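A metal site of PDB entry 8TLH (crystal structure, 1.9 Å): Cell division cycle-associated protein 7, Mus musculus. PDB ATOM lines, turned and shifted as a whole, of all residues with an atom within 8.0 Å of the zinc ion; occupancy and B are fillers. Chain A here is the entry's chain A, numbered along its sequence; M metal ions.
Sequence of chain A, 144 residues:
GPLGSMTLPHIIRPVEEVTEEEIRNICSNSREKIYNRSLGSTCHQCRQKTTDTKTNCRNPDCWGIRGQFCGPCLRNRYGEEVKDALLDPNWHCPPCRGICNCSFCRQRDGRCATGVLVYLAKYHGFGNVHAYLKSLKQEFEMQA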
ATOM      1  N   HIS A  44      12.628 -23.496   3.683  1.00  0.00           N
ATOM      2  CA  HIS A  44      11.526 -22.651   3.219  1.00  0.00           C
ATOM      3  C   HIS A  44      10.759 -23.313   2.082  1.00  0.00           C
ATOM      4  O   HIS A  44       9.529 -23.167   1.991  1.00  0.00           O
ATOM      5  CB  HIS A  44      12.064 -21.291   2.773  1.00  0.00           C
ATOM      6  CG  HIS A  44      11.037 -20.440   2.081  1.00  0.00           C
ATOM      7  ND1 HIS A  44       9.995 -19.838   2.751  1.00  0.00           N
ATOM      8  CD2 HIS A  44      10.909 -20.087   0.788  1.00  0.00           C
ATOM      9  CE1 HIS A  44       9.255 -19.154   1.890  1.00  0.00           C
ATOM     10  NE2 HIS A  44       9.795 -19.283   0.694  1.00  0.00           N
ATOM     11  N   GLN A  45      11.455 -24.042   1.208  1.00  0.00           N
ATOM     12  CA  GLN A  45      10.821 -24.568  -0.004  1.00  0.00           C
ATOM     13  C   GLN A  45       9.878 -25.721   0.330  1.00  0.00           C
ATOM     14  O   GLN A  45       8.682 -25.663   0.028  1.00  0.00           O
ATOM     15  CB  GLN A  45      11.890 -24.998  -1.001  1.00  0.00           C
ATOM     16  CG  GLN A  45      11.359 -25.357  -2.384  1.00  0.00           C
ATOM     17  CD  GLN A  45      11.120 -24.141  -3.254  1.00  0.00           C
ATOM     18  OE1 GLN A  45      11.565 -23.027  -2.943  1.00  0.00           O
ATOM     19  NE2 GLN A  45      10.418 -24.338  -4.364  1.00  0.00           N
ATOM     20  N   ARG A  47       9.283 -26.981   3.431  1.00  0.00           N
ATOM     21  CA  ARG A  47       8.626 -26.769   4.720  1.00  0.00           C
ATOM     22  C   ARG A  47       8.736 -27.997   5.626  1.00  0.00           C
ATOM     23  O   ARG A  47       7.821 -28.320   6.379  1.00  0.00           O
ATOM     24  CB  ARG A  47       7.171 -26.350   4.528  1.00  0.00           C
ATOM     25  CG  ARG A  47       7.040 -25.118   3.634  1.00  0.00           C
ATOM     26  CD  ARG A  47       5.624 -24.568   3.616  1.00  0.00           C
ATOM     27  NE  ARG A  47       4.715 -25.387   2.826  1.00  0.00           N
ATOM     28  CZ  ARG A  47       4.459 -25.198   1.543  1.00  0.00           C
ATOM     29  NH1 ARG A  47       5.042 -24.221   0.865  1.00  0.00           N
ATOM     30  NH2 ARG A  47       3.615 -26.015   0.923  1.00  0.00           N
ATOM     31  N   ARG A  66      13.069 -17.699   6.089  1.00  0.00           N
ATOM     32  CA  ARG A  66      12.829 -17.653   4.647  1.00  0.00           C
ATOM     33  C   ARG A  66      14.081 -17.913   3.831  1.00  0.00           C
ATOM     34  O   ARG A  66      13.982 -18.305   2.660  1.00  0.00           O
ATOM     35  CB  ARG A  66      12.217 -16.313   4.249  1.00  0.00           C
ATOM     36  CG  ARG A  66      13.142 -15.113   4.413  1.00  0.00           C
ATOM     37  CD  ARG A  66      12.365 -13.803   4.539  1.00  0.00           C
ATOM     38  NE  ARG A  66      11.757 -13.400   3.275  1.00  0.00           N
ATOM     39  CZ  ARG A  66      12.368 -12.681   2.345  1.00  0.00           C
ATOM     40  NH1 ARG A  66      13.613 -12.267   2.514  1.00  0.00           N
ATOM     41  NH2 ARG A  66      11.735 -12.384   1.227  1.00  0.00           N
ATOM     42  N   PHE A  69      17.298 -23.176   3.011  1.00  0.00           N
ATOM     43  CA  PHE A  69      16.954 -24.131   1.969  1.00  0.00           C
ATOM     44  C   PHE A  69      17.796 -25.377   2.124  1.00  0.00           C
ATOM     45  O   PHE A  69      19.003 -25.298   2.378  1.00  0.00           O
ATOM     46  CB  PHE A  69      17.160 -23.532   0.566  1.00  0.00           C
ATOM     47  CG  PHE A  69      16.141 -22.490   0.192  1.00  0.00           C
ATOM     48  CD1 PHE A  69      16.253 -21.182   0.649  1.00  0.00           C
ATOM     49  CD2 PHE A  69      15.064 -22.808  -0.631  1.00  0.00           C
ATOM     50  CE1 PHE A  69      15.316 -20.231   0.305  1.00  0.00           C
ATOM     51  CE2 PHE A  69      14.127 -21.858  -0.975  1.00  0.00           C
ATOM     52  CZ  PHE A  69      14.251 -20.561  -0.500  1.00  0.00           C
ATOM     53  N   TYR A  78      16.602 -24.217  -7.973  1.00  0.00           N
ATOM     54  CA  TYR A  78      17.365 -23.037  -8.322  1.00  0.00           C
ATOM     55  C   TYR A  78      18.721 -23.333  -8.947  1.00  0.00           C
ATOM     56  O   TYR A  78      19.433 -22.396  -9.325  1.00  0.00           O
ATOM     57  CB  TYR A  78      17.553 -22.140  -7.087  1.00  0.00           C
ATOM     58  CG  TYR A  78      16.231 -21.813  -6.429  1.00  0.00           C
ATOM     59  CD1 TYR A  78      15.420 -20.798  -6.922  1.00  0.00           C
ATOM     60  CD2 TYR A  78      15.770 -22.549  -5.349  1.00  0.00           C
ATOM     61  CE1 TYR A  78      14.206 -20.507  -6.337  1.00  0.00           C
ATOM     62  CE2 TYR A  78      14.560 -22.269  -4.757  1.00  0.00           C
ATOM     63  CZ  TYR A  78      13.787 -21.246  -5.251  1.00  0.00           C
ATOM     64  OH  TYR A  78      12.577 -20.966  -4.658  1.00  0.00           O
ATOM     65  N   PRO A  94      16.617 -16.960  -2.436  1.00  0.00           N
ATOM     66  CA  PRO A  94      15.702 -16.689  -3.562  1.00  0.00           C
ATOM     67  C   PRO A  94      14.562 -15.755  -3.164  1.00  0.00           C
ATOM     68  O   PRO A  94      14.167 -14.905  -3.976  1.00  0.00           O
ATOM     69  CB  PRO A  94      15.192 -18.083  -3.948  1.00  0.00           C
ATOM     70  CG  PRO A  94      16.305 -18.991  -3.577  1.00  0.00           C
ATOM     71  CD  PRO A  94      16.926 -18.401  -2.332  1.00  0.00           C
ATOM     72  N   PRO A  95      13.993 -15.872  -1.959  1.00  0.00           N
ATOM     73  CA  PRO A  95      13.018 -14.845  -1.544  1.00  0.00           C
ATOM     74  C   PRO A  95      13.597 -13.436  -1.546  1.00  0.00           C
ATOM     75  O   PRO A  95      12.907 -12.496  -1.948  1.00  0.00           O
ATOM     76  CB  PRO A  95      12.616 -15.289  -0.132  1.00  0.00           C
ATOM     77  CG  PRO A  95      12.754 -16.758  -0.176  1.00  0.00           C
ATOM     78  CD  PRO A  95      13.973 -17.010  -1.018  1.00  0.00           C
ATOM     79  N   ILE A  99      12.909 -14.444  -6.594  1.00  0.00           N
ATOM     80  CA  ILE A  99      12.765 -15.516  -7.567  1.00  0.00           C
ATOM     81  C   ILE A  99      12.323 -16.820  -6.924  1.00  0.00           C
ATOM     82  O   ILE A  99      12.450 -17.873  -7.535  1.00  0.00           O
ATOM     83  CB  ILE A  99      14.069 -15.729  -8.357  1.00  0.00           C
ATOM     84  CG1 ILE A  99      15.186 -16.204  -7.412  1.00  0.00           C
ATOM     85  CG2 ILE A  99      14.487 -14.463  -9.097  1.00  0.00           C
ATOM     86  CD1 ILE A  99      16.488 -16.539  -8.111  1.00  0.00           C
ATOM     87  N   CYS A 100      11.802 -16.776  -5.694  1.00  0.00           N
ATOM     88  CA  CYS A 100      11.384 -18.005  -5.040  1.00  0.00           C
ATOM     89  C   CYS A 100      10.184 -18.598  -5.751  1.00  0.00           C
ATOM     90  O   CYS A 100       9.228 -17.894  -6.076  1.00  0.00           O
ATOM     91  CB  CYS A 100      11.064 -17.768  -3.564  1.00  0.00           C
ATOM     92  SG  CYS A 100      10.727 -19.299  -2.653  1.00  0.00           S
ATOM     93  N   ASN A 101      10.232 -19.911  -6.005  1.00  0.00           N
ATOM     94  CA  ASN A 101       9.174 -20.597  -6.731  1.00  0.00           C
ATOM     95  C   ASN A 101       8.452 -21.619  -5.858  1.00  0.00           C
ATOM     96  O   ASN A 101       7.851 -22.557  -6.393  1.00  0.00           O
ATOM     97  CB  ASN A 101       9.723 -21.261  -8.001  1.00  0.00           C
ATOM     98  CG  ASN A 101      10.900 -22.191  -7.719  1.00  0.00           C
ATOM     99  OD1 ASN A 101      10.832 -23.065  -6.851  1.00  0.00           O
ATOM    100  ND2 ASN A 101      11.986 -22.000  -8.465  1.00  0.00           N
ATOM    101  N   CYS A 102       8.490 -21.454  -4.540  1.00  0.00           N
ATOM    102  CA  CYS A 102       7.720 -22.348  -3.683  1.00  0.00           C
ATOM    103  C   CYS A 102       6.229 -22.091  -3.880  1.00  0.00           C
ATOM    104  O   CYS A 102       5.813 -21.123  -4.518  1.00  0.00           O
ATOM    105  CB  CYS A 102       8.128 -22.167  -2.212  1.00  0.00           C
ATOM    106  SG  CYS A 102       7.447 -20.699  -1.382  1.00  0.00           S
ATOM    107  N   SER A 103       5.409 -22.980  -3.324  1.00  0.00           N
ATOM    108  CA  SER A 103       3.966 -22.904  -3.557  1.00  0.00           C
ATOM    109  C   SER A 103       3.406 -21.564  -3.073  1.00  0.00           C
ATOM    110  O   SER A 103       2.646 -20.911  -3.795  1.00  0.00           O
ATOM    111  CB  SER A 103       3.248 -24.064  -2.882  1.00  0.00           C
ATOM    112  OG  SER A 103       3.483 -24.092  -1.487  1.00  0.00           O
ATOM    113  N   PHE A 104       3.805 -21.135  -1.883  1.00  0.00           N
ATOM    114  CA  PHE A 104       3.275 -19.882  -1.344  1.00  0.00           C
ATOM    115  C   PHE A 104       3.776 -18.674  -2.130  1.00  0.00           C
ATOM    116  O   PHE A 104       2.979 -17.813  -2.508  1.00  0.00           O
ATOM    117  CB  PHE A 104       3.653 -19.751   0.140  1.00  0.00           C
ATOM    118  CG  PHE A 104       3.246 -18.443   0.741  1.00  0.00           C
ATOM    119  CD1 PHE A 104       1.941 -18.222   1.157  1.00  0.00           C
ATOM    120  CD2 PHE A 104       4.167 -17.420   0.905  1.00  0.00           C
ATOM    121  CE1 PHE A 104       1.565 -17.015   1.718  1.00  0.00           C
ATOM    122  CE2 PHE A 104       3.801 -16.210   1.466  1.00  0.00           C
ATOM    123  CZ  PHE A 104       2.500 -16.009   1.877  1.00  0.00           C
ATOM    124  N   CYS A 105       5.083 -18.601  -2.392  1.00  0.00           N
ATOM    125  CA  CYS A 105       5.642 -17.409  -3.031  1.00  0.00           C
ATOM    126  C   CYS A 105       5.134 -17.256  -4.457  1.00  0.00           C
ATOM    127  O   CYS A 105       4.812 -16.131  -4.880  1.00  0.00           O
ATOM    128  CB  CYS A 105       7.168 -17.462  -2.993  1.00  0.00           C
ATOM    129  SG  CYS A 105       7.858 -17.054  -1.367  1.00  0.00           S
ATOM    130  N   ARG A 106       5.050 -18.346  -5.213  1.00  0.00           N
ATOM    131  CA  ARG A 106       4.495 -18.249  -6.555  1.00  0.00           C
ATOM    132  C   ARG A 106       2.974 -18.163  -6.547  1.00  0.00           C
ATOM    133  O   ARG A 106       2.385 -17.772  -7.560  1.00  0.00           O
ATOM    134  CB  ARG A 106       4.949 -19.425  -7.421  1.00  0.00           C
ATOM    135  CG  ARG A 106       4.187 -20.717  -7.194  1.00  0.00           C
ATOM    136  CD  ARG A 106       4.692 -21.807  -8.129  1.00  0.00           C
ATOM    137  NE  ARG A 106       3.936 -23.042  -7.974  1.00  0.00           N
ATOM    138  CZ  ARG A 106       4.313 -24.047  -7.187  1.00  0.00           C
ATOM    139  NH1 ARG A 106       5.425 -24.000  -6.485  1.00  0.00           N
ATOM    140  NH2 ARG A 106       3.533 -25.129  -7.105  1.00  0.00           N
ATOM    141  N   GLN A 107       2.331 -18.518  -5.430  1.00  0.00           N
ATOM    142  CA  GLN A 107       0.888 -18.310  -5.314  1.00  0.00           C
ATOM    143  C   GLN A 107       0.544 -16.828  -5.235  1.00  0.00           C
ATOM    144  O   GLN A 107      -0.509 -16.411  -5.747  1.00  0.00           O
ATOM    145  CB  GLN A 107       0.349 -19.047  -4.097  1.00  0.00           C
ATOM    146  N   ARG A 108       1.399 -16.019  -4.617  1.00  0.00           N
ATOM    147  CA  ARG A 108       1.177 -14.577  -4.523  1.00  0.00           C
ATOM    148  C   ARG A 108       1.312 -13.935  -5.903  1.00  0.00           C
ATOM    149  O   ARG A 108       2.414 -13.689  -6.376  1.00  0.00           O
ATOM    150  CB  ARG A 108       2.158 -13.932  -3.555  1.00  0.00           C
ATOM    151  CG  ARG A 108       2.334 -14.655  -2.228  1.00  0.00           C
ATOM    152  CD  ARG A 108       3.052 -13.775  -1.203  1.00  0.00           C
ATOM    153  NE  ARG A 108       4.063 -12.927  -1.829  1.00  0.00           N
ATOM    154  CZ  ARG A 108       5.347 -13.258  -1.957  1.00  0.00           C
ATOM    155  NH1 ARG A 108       5.808 -14.411  -1.507  1.00  0.00           N
ATOM    156  NH2 ARG A 108       6.173 -12.403  -2.550  1.00  0.00           N
HETATM  157 ZN    ZN M   1       9.016 -19.012  -1.163  1.00  0.00          ZN
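SG of Cys 105 sits close to NH1 of Arg 108, at 3.3 Å. The side-chain sulfur (SG) of Cys 100 sits close to the side-chain hydroxyl (OH) of Tyr 78 (3.2 Å). N of Cys 100 lies within hydrogen-bond range of O of Pro 94, 3.5 Å away. The backbone NH (N) of Cys 102 sits close to the side-chain amide nitrogen (NE2) of Gln 45 (3.5 Å). The backbone NH of Phe 104 sits close to the side-chain sulfur of Cys 102.
Of the 18 residues printed, 4 come within 4 Å of the zinc ion.
The zinc ion is bound by a ring nitrogen (NE2) of His 44 (2.0 Å), the side-chain sulfur (SG) of Cys 105 (2.3 Å), the side-chain sulfur (SG) of Cys 100 (2.3 Å) and the side-chain sulfur (SG) of Cys 102 (2.3 Å).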
